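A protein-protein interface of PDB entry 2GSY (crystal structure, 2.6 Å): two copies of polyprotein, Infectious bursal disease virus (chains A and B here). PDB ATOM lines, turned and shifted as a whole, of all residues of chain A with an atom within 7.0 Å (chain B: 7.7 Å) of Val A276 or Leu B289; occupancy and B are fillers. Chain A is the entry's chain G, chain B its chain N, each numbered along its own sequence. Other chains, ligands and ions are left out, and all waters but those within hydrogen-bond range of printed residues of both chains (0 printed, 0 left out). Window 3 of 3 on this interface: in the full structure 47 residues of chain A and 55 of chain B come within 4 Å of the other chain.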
ATOM      1  N   VAL A 242       4.840 -28.365 -20.988  1.00  0.00           N
ATOM      2  CA  VAL A 242       3.637 -29.083 -20.583  1.00  0.00           C
ATOM      3  C   VAL A 242       2.426 -28.365 -21.159  1.00  0.00           C
ATOM      4  O   VAL A 242       2.255 -27.165 -20.960  1.00  0.00           O
ATOM      5  CB  VAL A 242       3.508 -29.174 -19.042  1.00  0.00           C
ATOM      6  CG1 VAL A 242       2.325 -30.045 -18.650  1.00  0.00           C
ATOM      7  CG2 VAL A 242       4.788 -29.724 -18.424  1.00  0.00           C
ATOM      8  N   GLY A 258      -6.122 -24.244  -6.293  1.00  0.00           N
ATOM      9  CA  GLY A 258      -4.710 -24.004  -6.544  1.00  0.00           C
ATOM     10  C   GLY A 258      -4.124 -25.271  -7.132  1.00  0.00           C
ATOM     11  O   GLY A 258      -4.529 -26.374  -6.764  1.00  0.00           O
ATOM     12  N   ALA A 259      -3.184 -25.119  -8.058  1.00  0.00           N
ATOM     13  CA  ALA A 259      -2.543 -26.267  -8.675  1.00  0.00           C
ATOM     14  C   ALA A 259      -1.098 -25.963  -9.035  1.00  0.00           C
ATOM     15  O   ALA A 259      -0.786 -24.902  -9.577  1.00  0.00           O
ATOM     16  CB  ALA A 259      -3.316 -26.719  -9.896  1.00  0.00           C
ATOM     17  N   THR A 260      -0.226 -26.912  -8.725  1.00  0.00           N
ATOM     18  CA  THR A 260       1.203 -26.744  -8.915  1.00  0.00           C
ATOM     19  C   THR A 260       1.778 -27.989  -9.563  1.00  0.00           C
ATOM     20  O   THR A 260       1.394 -29.112  -9.231  1.00  0.00           O
ATOM     21  CB  THR A 260       1.915 -26.481  -7.567  1.00  0.00           C
ATOM     22  OG1 THR A 260       1.337 -25.333  -6.936  1.00  0.00           O
ATOM     23  CG2 THR A 260       3.402 -26.235  -7.768  1.00  0.00           C
ATOM     24  N   ILE A 261       2.691 -27.777 -10.500  1.00  0.00           N
ATOM     25  CA  ILE A 261       3.432 -28.871 -11.090  1.00  0.00           C
ATOM     26  C   ILE A 261       4.835 -28.924 -10.516  1.00  0.00           C
ATOM     27  O   ILE A 261       5.520 -27.904 -10.417  1.00  0.00           O
ATOM     28  CB  ILE A 261       3.438 -28.790 -12.624  1.00  0.00           C
ATOM     29  CG1 ILE A 261       2.155 -29.447 -13.139  1.00  0.00           C
ATOM     30  CG2 ILE A 261       4.700 -29.436 -13.211  1.00  0.00           C
ATOM     31  CD1 ILE A 261       2.210 -29.922 -14.547  1.00  0.00           C
ATOM     32  N   ARG A 274       6.277 -25.211 -10.420  1.00  0.00           N
ATOM     33  CA  ARG A 274       5.530 -24.183 -11.151  1.00  0.00           C
ATOM     34  C   ARG A 274       4.049 -24.170 -10.826  1.00  0.00           C
ATOM     35  O   ARG A 274       3.335 -25.144 -11.090  1.00  0.00           O
ATOM     36  CB  ARG A 274       5.701 -24.339 -12.663  1.00  0.00           C
ATOM     37  CG  ARG A 274       7.115 -24.142 -13.161  1.00  0.00           C
ATOM     38  CD  ARG A 274       7.622 -22.710 -12.975  1.00  0.00           C
ATOM     39  NE  ARG A 274       8.847 -22.494 -13.747  1.00  0.00           N
ATOM     40  CZ  ARG A 274       8.876 -22.302 -15.067  1.00  0.00           C
ATOM     41  NH1 ARG A 274       7.746 -22.291 -15.772  1.00  0.00           N
ATOM     42  NH2 ARG A 274      10.036 -22.117 -15.688  1.00  0.00           N
ATOM     43  N   ALA A 275       3.592 -23.055 -10.264  1.00  0.00           N
ATOM     44  CA  ALA A 275       2.173 -22.854 -10.031  1.00  0.00           C
ATOM     45  C   ALA A 275       1.479 -22.771 -11.386  1.00  0.00           C
ATOM     46  O   ALA A 275       1.840 -21.948 -12.231  1.00  0.00           O
ATOM     47  CB  ALA A 275       1.944 -21.602  -9.223  1.00  0.00           C
ATOM     48  N   VAL A 276       0.510 -23.654 -11.597  1.00  0.00           N
ATOM     49  CA  VAL A 276      -0.204 -23.747 -12.866  1.00  0.00           C
ATOM     50  C   VAL A 276      -1.495 -22.940 -12.812  1.00  0.00           C
ATOM     51  O   VAL A 276      -1.949 -22.400 -13.823  1.00  0.00           O
ATOM     52  CB  VAL A 276      -0.490 -25.213 -13.213  1.00  0.00           C
ATOM     53  CG1 VAL A 276      -1.580 -25.329 -14.261  1.00  0.00           C
ATOM     54  CG2 VAL A 276       0.783 -25.880 -13.696  1.00  0.00           C
ATOM     55  N   ALA A 277      -2.082 -22.877 -11.625  1.00  0.00           N
ATOM     56  CA  ALA A 277      -3.215 -22.017 -11.360  1.00  0.00           C
ATOM     57  C   ALA A 277      -3.274 -21.825  -9.860  1.00  0.00           C
ATOM     58  O   ALA A 277      -3.372 -22.794  -9.111  1.00  0.00           O
ATOM     59  CB  ALA A 277      -4.507 -22.644 -11.879  1.00  0.00           C
ATOM     60  N   ALA A 278      -3.165 -20.581  -9.416  1.00  0.00           N
ATOM     61  CA  ALA A 278      -3.328 -20.273  -8.006  1.00  0.00           C
ATOM     62  C   ALA A 278      -4.592 -19.453  -7.877  1.00  0.00           C
ATOM     63  O   ALA A 278      -4.958 -18.744  -8.816  1.00  0.00           O
ATOM     64  CB  ALA A 278      -2.126 -19.510  -7.475  1.00  0.00           C
ATOM     65  N   ASN A 280      -8.337 -19.659  -7.881  1.00  0.00           N
ATOM     66  CA  ASN A 280      -9.069 -19.871  -9.122  1.00  0.00           C
ATOM     67  C   ASN A 280     -10.478 -20.359  -8.795  1.00  0.00           C
ATOM     68  O   ASN A 280     -10.690 -21.548  -8.536  1.00  0.00           O
ATOM     69  CB  ASN A 280      -8.311 -20.895  -9.981  1.00  0.00           C
ATOM     70  CG  ASN A 280      -8.925 -21.104 -11.359  1.00  0.00           C
ATOM     71  OD1 ASN A 280     -10.101 -20.820 -11.594  1.00  0.00           O
ATOM     72  ND2 ASN A 280      -8.121 -21.623 -12.278  1.00  0.00           N
ATOM     73  N   MET A 290      -8.708 -25.304 -16.684  1.00  0.00           N
ATOM     74  CA  MET A 290      -7.393 -25.088 -16.119  1.00  0.00           C
ATOM     75  C   MET A 290      -6.353 -25.479 -17.160  1.00  0.00           C
ATOM     76  O   MET A 290      -5.956 -26.641 -17.241  1.00  0.00           O
ATOM     77  CB  MET A 290      -7.218 -25.905 -14.847  1.00  0.00           C
ATOM     78  CG  MET A 290      -5.970 -25.560 -14.075  1.00  0.00           C
ATOM     79  SD  MET A 290      -5.932 -26.408 -12.498  1.00  0.00           S
ATOM     80  CE  MET A 290      -5.013 -27.861 -12.943  1.00  0.00           C
ATOM     81  N   PRO A 291      -5.907 -24.499 -17.964  1.00  0.00           N
ATOM     82  CA  PRO A 291      -4.972 -24.785 -19.040  1.00  0.00           C
ATOM     83  C   PRO A 291      -3.563 -24.991 -18.511  1.00  0.00           C
ATOM     84  O   PRO A 291      -3.223 -24.513 -17.430  1.00  0.00           O
ATOM     85  CB  PRO A 291      -5.018 -23.518 -19.904  1.00  0.00           C
ATOM     86  CG  PRO A 291      -6.027 -22.616 -19.282  1.00  0.00           C
ATOM     87  CD  PRO A 291      -6.232 -23.067 -17.891  1.00  0.00           C
ATOM     88  N   PHE A 292      -2.756 -25.711 -19.275  1.00  0.00           N
ATOM     89  CA  PHE A 292      -1.357 -25.887 -18.952  1.00  0.00           C
ATOM     90  C   PHE A 292      -0.532 -25.279 -20.069  1.00  0.00           C
ATOM     91  O   PHE A 292      -0.613 -25.708 -21.219  1.00  0.00           O
ATOM     92  CB  PHE A 292      -1.037 -27.368 -18.757  1.00  0.00           C
ATOM     93  CG  PHE A 292      -1.525 -27.915 -17.451  1.00  0.00           C
ATOM     94  CD1 PHE A 292      -2.887 -28.071 -17.208  1.00  0.00           C
ATOM     95  CD2 PHE A 292      -0.627 -28.260 -16.454  1.00  0.00           C
ATOM     96  CE1 PHE A 292      -3.344 -28.567 -15.996  1.00  0.00           C
ATOM     97  CE2 PHE A 292      -1.076 -28.761 -15.238  1.00  0.00           C
ATOM     98  CZ  PHE A 292      -2.436 -28.914 -15.009  1.00  0.00           C
ATOM     99  N   ASN A 293       0.232 -24.250 -19.725  1.00  0.00           N
ATOM    100  CA  ASN A 293       1.068 -23.548 -20.687  1.00  0.00           C
ATOM    101  C   ASN A 293       2.483 -23.394 -20.150  1.00  0.00           C
ATOM    102  O   ASN A 293       2.998 -22.281 -20.061  1.00  0.00           O
ATOM    103  CB  ASN A 293       0.477 -22.170 -20.989  1.00  0.00           C
ATOM    104  CG  ASN A 293      -0.920 -22.246 -21.573  1.00  0.00           C
ATOM    105  OD1 ASN A 293      -1.100 -22.655 -22.719  1.00  0.00           O
ATOM    106  ND2 ASN A 293      -1.918 -21.832 -20.790  1.00  0.00           N
ATOM    107  N   LEU A 294       3.111 -24.506 -19.788  1.00  0.00           N
ATOM    108  CA  LEU A 294       4.420 -24.442 -19.154  1.00  0.00           C
ATOM    109  C   LEU A 294       5.536 -24.646 -20.140  1.00  0.00           C
ATOM    110  O   LEU A 294       5.499 -25.569 -20.943  1.00  0.00           O
ATOM    111  CB  LEU A 294       4.557 -25.489 -18.053  1.00  0.00           C
ATOM    112  CG  LEU A 294       3.593 -25.462 -16.876  1.00  0.00           C
ATOM    113  CD1 LEU A 294       4.099 -26.432 -15.826  1.00  0.00           C
ATOM    114  CD2 LEU A 294       3.458 -24.056 -16.304  1.00  0.00           C
ATOM    115  N   LEU A 310       1.453 -33.461 -10.108  1.00  0.00           N
ATOM    116  CA  LEU A 310       0.560 -32.328 -10.023  1.00  0.00           C
ATOM    117  C   LEU A 310      -0.206 -32.370  -8.713  1.00  0.00           C
ATOM    118  O   LEU A 310      -0.892 -33.348  -8.418  1.00  0.00           O
ATOM    119  CB  LEU A 310      -0.412 -32.332 -11.201  1.00  0.00           C
ATOM    120  CG  LEU A 310      -1.572 -31.336 -11.154  1.00  0.00           C
ATOM    121  CD1 LEU A 310      -1.096 -29.917 -11.412  1.00  0.00           C
ATOM    122  CD2 LEU A 310      -2.617 -31.740 -12.163  1.00  0.00           C
ATOM    123  N   GLU A 311      -0.075 -31.308  -7.929  1.00  0.00           N
ATOM    124  CA  GLU A 311      -0.842 -31.165  -6.705  1.00  0.00           C
ATOM    125  C   GLU A 311      -1.954 -30.161  -6.917  1.00  0.00           C
ATOM    126  O   GLU A 311      -1.791 -29.196  -7.659  1.00  0.00           O
ATOM    127  CB  GLU A 311       0.050 -30.719  -5.549  1.00  0.00           C
ATOM    128  CG  GLU A 311       0.883 -31.842  -4.955  1.00  0.00           C
ATOM    129  CD  GLU A 311       1.685 -31.420  -3.736  1.00  0.00           C
ATOM    130  OE1 GLU A 311       1.370 -30.377  -3.115  1.00  0.00           O
ATOM    131  OE2 GLU A 311       2.642 -32.149  -3.398  1.00  0.00           O
ATOM    132  N   GLU B 245       4.059 -18.999 -20.890  1.00  0.00           N
ATOM    133  CA  GLU B 245       3.272 -18.197 -19.972  1.00  0.00           C
ATOM    134  C   GLU B 245       4.134 -17.229 -19.190  1.00  0.00           C
ATOM    135  O   GLU B 245       5.222 -17.580 -18.734  1.00  0.00           O
ATOM    136  CB  GLU B 245       2.570 -19.126 -18.993  1.00  0.00           C
ATOM    137  CG  GLU B 245       1.355 -18.547 -18.323  1.00  0.00           C
ATOM    138  CD  GLU B 245       0.600 -19.602 -17.539  1.00  0.00           C
ATOM    139  OE1 GLU B 245       1.255 -20.397 -16.824  1.00  0.00           O
ATOM    140  OE2 GLU B 245      -0.648 -19.640 -17.647  1.00  0.00           O
ATOM    141  N   LEU B 246       3.641 -16.008 -19.042  1.00  0.00           N
ATOM    142  CA  LEU B 246       4.217 -15.079 -18.093  1.00  0.00           C
ATOM    143  C   LEU B 246       3.294 -14.990 -16.896  1.00  0.00           C
ATOM    144  O   LEU B 246       2.073 -15.081 -17.030  1.00  0.00           O
ATOM    145  CB  LEU B 246       4.427 -13.704 -18.719  1.00  0.00           C
ATOM    146  CG  LEU B 246       5.460 -13.631 -19.844  1.00  0.00           C
ATOM    147  CD1 LEU B 246       5.509 -12.236 -20.407  1.00  0.00           C
ATOM    148  CD2 LEU B 246       6.837 -14.048 -19.356  1.00  0.00           C
ATOM    149  N   VAL B 247       3.893 -14.834 -15.723  1.00  0.00           N
ATOM    150  CA  VAL B 247       3.158 -14.711 -14.478  1.00  0.00           C
ATOM    151  C   VAL B 247       3.498 -13.356 -13.870  1.00  0.00           C
ATOM    152  O   VAL B 247       4.672 -13.013 -13.717  1.00  0.00           O
ATOM    153  CB  VAL B 247       3.524 -15.851 -13.501  1.00  0.00           C
ATOM    154  CG1 VAL B 247       2.848 -15.653 -12.155  1.00  0.00           C
ATOM    155  CG2 VAL B 247       3.149 -17.205 -14.091  1.00  0.00           C
ATOM    156  N   PHE B 248       2.464 -12.590 -13.534  1.00  0.00           N
ATOM    157  CA  PHE B 248       2.637 -11.253 -12.981  1.00  0.00           C
ATOM    158  C   PHE B 248       2.160 -11.166 -11.539  1.00  0.00           C
ATOM    159  O   PHE B 248       1.100 -11.691 -11.200  1.00  0.00           O
ATOM    160  CB  PHE B 248       1.891 -10.228 -13.834  1.00  0.00           C
ATOM    161  CG  PHE B 248       2.447 -10.070 -15.218  1.00  0.00           C
ATOM    162  CD1 PHE B 248       2.000 -10.874 -16.260  1.00  0.00           C
ATOM    163  CD2 PHE B 248       3.412  -9.107 -15.485  1.00  0.00           C
ATOM    164  CE1 PHE B 248       2.512 -10.722 -17.548  1.00  0.00           C
ATOM    165  CE2 PHE B 248       3.927  -8.948 -16.765  1.00  0.00           C
ATOM    166  CZ  PHE B 248       3.479  -9.757 -17.798  1.00  0.00           C
ATOM    167  N   ARG B 249       2.953 -10.504 -10.700  1.00  0.00           N
ATOM    168  CA  ARG B 249       2.589 -10.233  -9.307  1.00  0.00           C
ATOM    169  C   ARG B 249       2.584  -8.727  -9.089  1.00  0.00           C
ATOM    170  O   ARG B 249       3.343  -8.007  -9.734  1.00  0.00           O
ATOM    171  CB  ARG B 249       3.604 -10.855  -8.344  1.00  0.00           C
ATOM    172  CG  ARG B 249       3.967 -12.312  -8.598  1.00  0.00           C
ATOM    173  CD  ARG B 249       3.103 -13.274  -7.808  1.00  0.00           C
ATOM    174  NE  ARG B 249       3.093 -12.976  -6.380  1.00  0.00           N
ATOM    175  CZ  ARG B 249       2.383 -13.648  -5.477  1.00  0.00           C
ATOM    176  NH1 ARG B 249       1.625 -14.671  -5.849  1.00  0.00           N
ATOM    177  NH2 ARG B 249       2.431 -13.297  -4.200  1.00  0.00           N
ATOM    178  N   ALA B 277      -2.535 -10.360 -24.972  1.00  0.00           N
ATOM    179  CA  ALA B 277      -3.502 -10.065 -23.933  1.00  0.00           C
ATOM    180  C   ALA B 277      -3.739  -8.571 -23.973  1.00  0.00           C
ATOM    181  O   ALA B 277      -2.804  -7.788 -23.830  1.00  0.00           O
ATOM    182  CB  ALA B 277      -2.982 -10.494 -22.563  1.00  0.00           C
ATOM    183  N   ASN B 280      -6.394  -6.404 -19.233  1.00  0.00           N
ATOM    184  CA  ASN B 280      -6.215  -7.599 -18.418  1.00  0.00           C
ATOM    185  C   ASN B 280      -5.863  -7.189 -16.991  1.00  0.00           C
ATOM    186  O   ASN B 280      -4.705  -6.886 -16.690  1.00  0.00           O
ATOM    187  CB  ASN B 280      -5.103  -8.463 -19.037  1.00  0.00           C
ATOM    188  CG  ASN B 280      -4.913  -9.801 -18.336  1.00  0.00           C
ATOM    189  OD1 ASN B 280      -5.298  -9.986 -17.178  1.00  0.00           O
ATOM    190  ND2 ASN B 280      -4.299 -10.743 -19.043  1.00  0.00           N
ATOM    191  N   GLY B 281      -6.872  -7.172 -16.123  1.00  0.00           N
ATOM    192  CA  GLY B 281      -6.709  -6.716 -14.745  1.00  0.00           C
ATOM    193  C   GLY B 281      -5.805  -7.615 -13.925  1.00  0.00           C
ATOM    194  O   GLY B 281      -5.856  -8.839 -14.051  1.00  0.00           O
ATOM    195  N   LEU B 282      -4.965  -6.998 -13.098  1.00  0.00           N
ATOM    196  CA  LEU B 282      -4.091  -7.734 -12.190  1.00  0.00           C
ATOM    197  C   LEU B 282      -4.642  -7.682 -10.774  1.00  0.00           C
ATOM    198  O   LEU B 282      -4.985  -6.611 -10.273  1.00  0.00           O
ATOM    199  CB  LEU B 282      -2.664  -7.171 -12.210  1.00  0.00           C
ATOM    200  CG  LEU B 282      -1.875  -7.075 -13.520  1.00  0.00           C
ATOM    201  CD1 LEU B 282      -0.504  -6.486 -13.253  1.00  0.00           C
ATOM    202  CD2 LEU B 282      -1.740  -8.421 -14.209  1.00  0.00           C
ATOM    203  N   THR B 286      -1.557 -12.396  -5.835  1.00  0.00           N
ATOM    204  CA  THR B 286      -1.805 -13.646  -6.552  1.00  0.00           C
ATOM    205  C   THR B 286      -0.983 -13.670  -7.829  1.00  0.00           C
ATOM    206  O   THR B 286      -0.598 -12.620  -8.346  1.00  0.00           O
ATOM    207  CB  THR B 286      -3.293 -13.798  -6.952  1.00  0.00           C
ATOM    208  OG1 THR B 286      -4.131 -13.369  -5.879  1.00  0.00           O
ATOM    209  CG2 THR B 286      -3.629 -15.248  -7.296  1.00  0.00           C
ATOM    210  N   ASP B 287      -0.715 -14.873  -8.329  1.00  0.00           N
ATOM    211  CA  ASP B 287      -0.206 -15.036  -9.678  1.00  0.00           C
ATOM    212  C   ASP B 287      -1.284 -14.584 -10.662  1.00  0.00           C
ATOM    213  O   ASP B 287      -2.458 -14.940 -10.521  1.00  0.00           O
ATOM    214  CB  ASP B 287       0.173 -16.500  -9.943  1.00  0.00           C
ATOM    215  CG  ASP B 287       1.357 -16.974  -9.097  1.00  0.00           C
ATOM    216  OD1 ASP B 287       2.286 -16.181  -8.834  1.00  0.00           O
ATOM    217  OD2 ASP B 287       1.362 -18.160  -8.704  1.00  0.00           O
ATOM    218  N   ASN B 288      -0.880 -13.768 -11.632  1.00  0.00           N
ATOM    219  CA  ASN B 288      -1.739 -13.377 -12.741  1.00  0.00           C
ATOM    220  C   ASN B 288      -1.158 -13.945 -14.020  1.00  0.00           C
ATOM    221  O   ASN B 288      -0.080 -13.535 -14.460  1.00  0.00           O
ATOM    222  CB  ASN B 288      -1.846 -11.858 -12.841  1.00  0.00           C
ATOM    223  CG  ASN B 288      -2.630 -11.257 -11.700  1.00  0.00           C
ATOM    224  OD1 ASN B 288      -2.065 -10.891 -10.669  1.00  0.00           O
ATOM    225  ND2 ASN B 288      -3.942 -11.164 -11.869  1.00  0.00           N
ATOM    226  N   LEU B 289      -1.870 -14.899 -14.608  1.00  0.00           N
ATOM    227  CA  LEU B 289      -1.338 -15.655 -15.730  1.00  0.00           C
ATOM    228  C   LEU B 289      -1.577 -14.954 -17.048  1.00  0.00           C
ATOM    229  O   LEU B 289      -2.645 -14.389 -17.281  1.00  0.00           O
ATOM    230  CB  LEU B 289      -1.944 -17.057 -15.779  1.00  0.00           C
ATOM    231  CG  LEU B 289      -1.937 -17.923 -14.516  1.00  0.00           C
ATOM    232  CD1 LEU B 289      -2.695 -19.207 -14.793  1.00  0.00           C
ATOM    233  CD2 LEU B 289      -0.523 -18.222 -14.029  1.00  0.00           C
ATOM    234  N   MET B 290      -0.565 -14.995 -17.902  1.00  0.00           N
ATOM    235  CA  MET B 290      -0.682 -14.505 -19.257  1.00  0.00           C
ATOM    236  C   MET B 290      -0.173 -15.582 -20.203  1.00  0.00           C
ATOM    237  O   MET B 290       1.022 -15.646 -20.493  1.00  0.00           O
ATOM    238  CB  MET B 290       0.112 -13.218 -19.429  1.00  0.00           C
ATOM    239  CG  MET B 290      -0.145 -12.519 -20.742  1.00  0.00           C
ATOM    240  SD  MET B 290       0.661 -10.918 -20.788  1.00  0.00           S
ATOM    241  CE  MET B 290       2.202 -11.368 -21.553  1.00  0.00           C
ATOM    242  N   PRO B 291      -1.084 -16.439 -20.688  1.00  0.00           N
ATOM    243  CA  PRO B 291      -0.686 -17.550 -21.536  1.00  0.00           C
ATOM    244  C   PRO B 291      -0.372 -17.087 -22.949  1.00  0.00           C
ATOM    245  O   PRO B 291      -0.854 -16.042 -23.388  1.00  0.00           O
ATOM    246  CB  PRO B 291      -1.926 -18.453 -21.557  1.00  0.00           C
ATOM    247  CG  PRO B 291      -2.935 -17.811 -20.661  1.00  0.00           C
ATOM    248  CD  PRO B 291      -2.541 -16.395 -20.491  1.00  0.00           C
ATOM    249  N   PHE B 292       0.442 -17.865 -23.647  1.00  0.00           N
ATOM    250  CA  PHE B 292       0.729 -17.612 -25.042  1.00  0.00           C
ATOM    251  C   PHE B 292       0.226 -18.788 -25.856  1.00  0.00           C
ATOM    252  O   PHE B 292       0.676 -19.919 -25.674  1.00  0.00           O
ATOM    253  CB  PHE B 292       2.224 -17.386 -25.240  1.00  0.00           C
ATOM    254  CG  PHE B 292       2.690 -16.040 -24.776  1.00  0.00           C
ATOM    255  CD1 PHE B 292       2.717 -15.722 -23.421  1.00  0.00           C
ATOM    256  CD2 PHE B 292       3.090 -15.081 -25.692  1.00  0.00           C
ATOM    257  CE1 PHE B 292       3.136 -14.475 -22.988  1.00  0.00           C
ATOM    258  CE2 PHE B 292       3.514 -13.829 -25.268  1.00  0.00           C
ATOM    259  CZ  PHE B 292       3.536 -13.527 -23.913  1.00  0.00           C
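The backbone carbonyl oxygen (O) of Ala A259 is in hydrogen-bond range of the backbone NH (N) of Val A276. The guanidinium group (NH1) of Arg B249 lies within salt-bridge range of the side-chain carboxylate (OD1) of Asp B287 (3.4 Å).
Printed residues of chain B that touch a printed residue of chain A: Glu B245, Asp B287, Leu B289 and Pro B291. Of the 18 printed residues of chain A, 4 touch a printed residue of chain B. Hydrophobic or aromatic side chains of chain A that line the printed part of chain B: Ala A275 and Ala A278. Among the printed residues, no Asp or Glu carboxylate lies within 4 Å of a Lys or Arg side-chain nitrogen of the other chain.
Ala A275 touches Asp B287. CD1 of Leu B289 touches O of Val A276 (3.4 Å). CB of Ala A278 touches OD2 of Asp B287, 3.9 Å away. Glu B245 touches Asn A293 (CB to O, 3.4 Å). Pro B291 touches Asn A293.
5 positions are printed for both chains.
Of the printed residues of chain B, Val A276 touches Leu B289. Of chain A, only Val A276 comes within 4 Å of Leu B289. Ala A275 touches just one residue of chain B: Asp B287 (3.5 Å). Of the printed residues of chain B, Asn A293 touches Glu B245 (3.4 Å) and Pro B291 (3.5 Å). Of the printed residues of chain A, Asp B287 touches Ala A275 and Ala A278. Ile A261 touches none of the printed residues of chain B. Leu B282 touches none of the printed residues of chain A. The nearest residue of chain A that does not touch Leu B289 is Ala A277 (4.5 Å).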
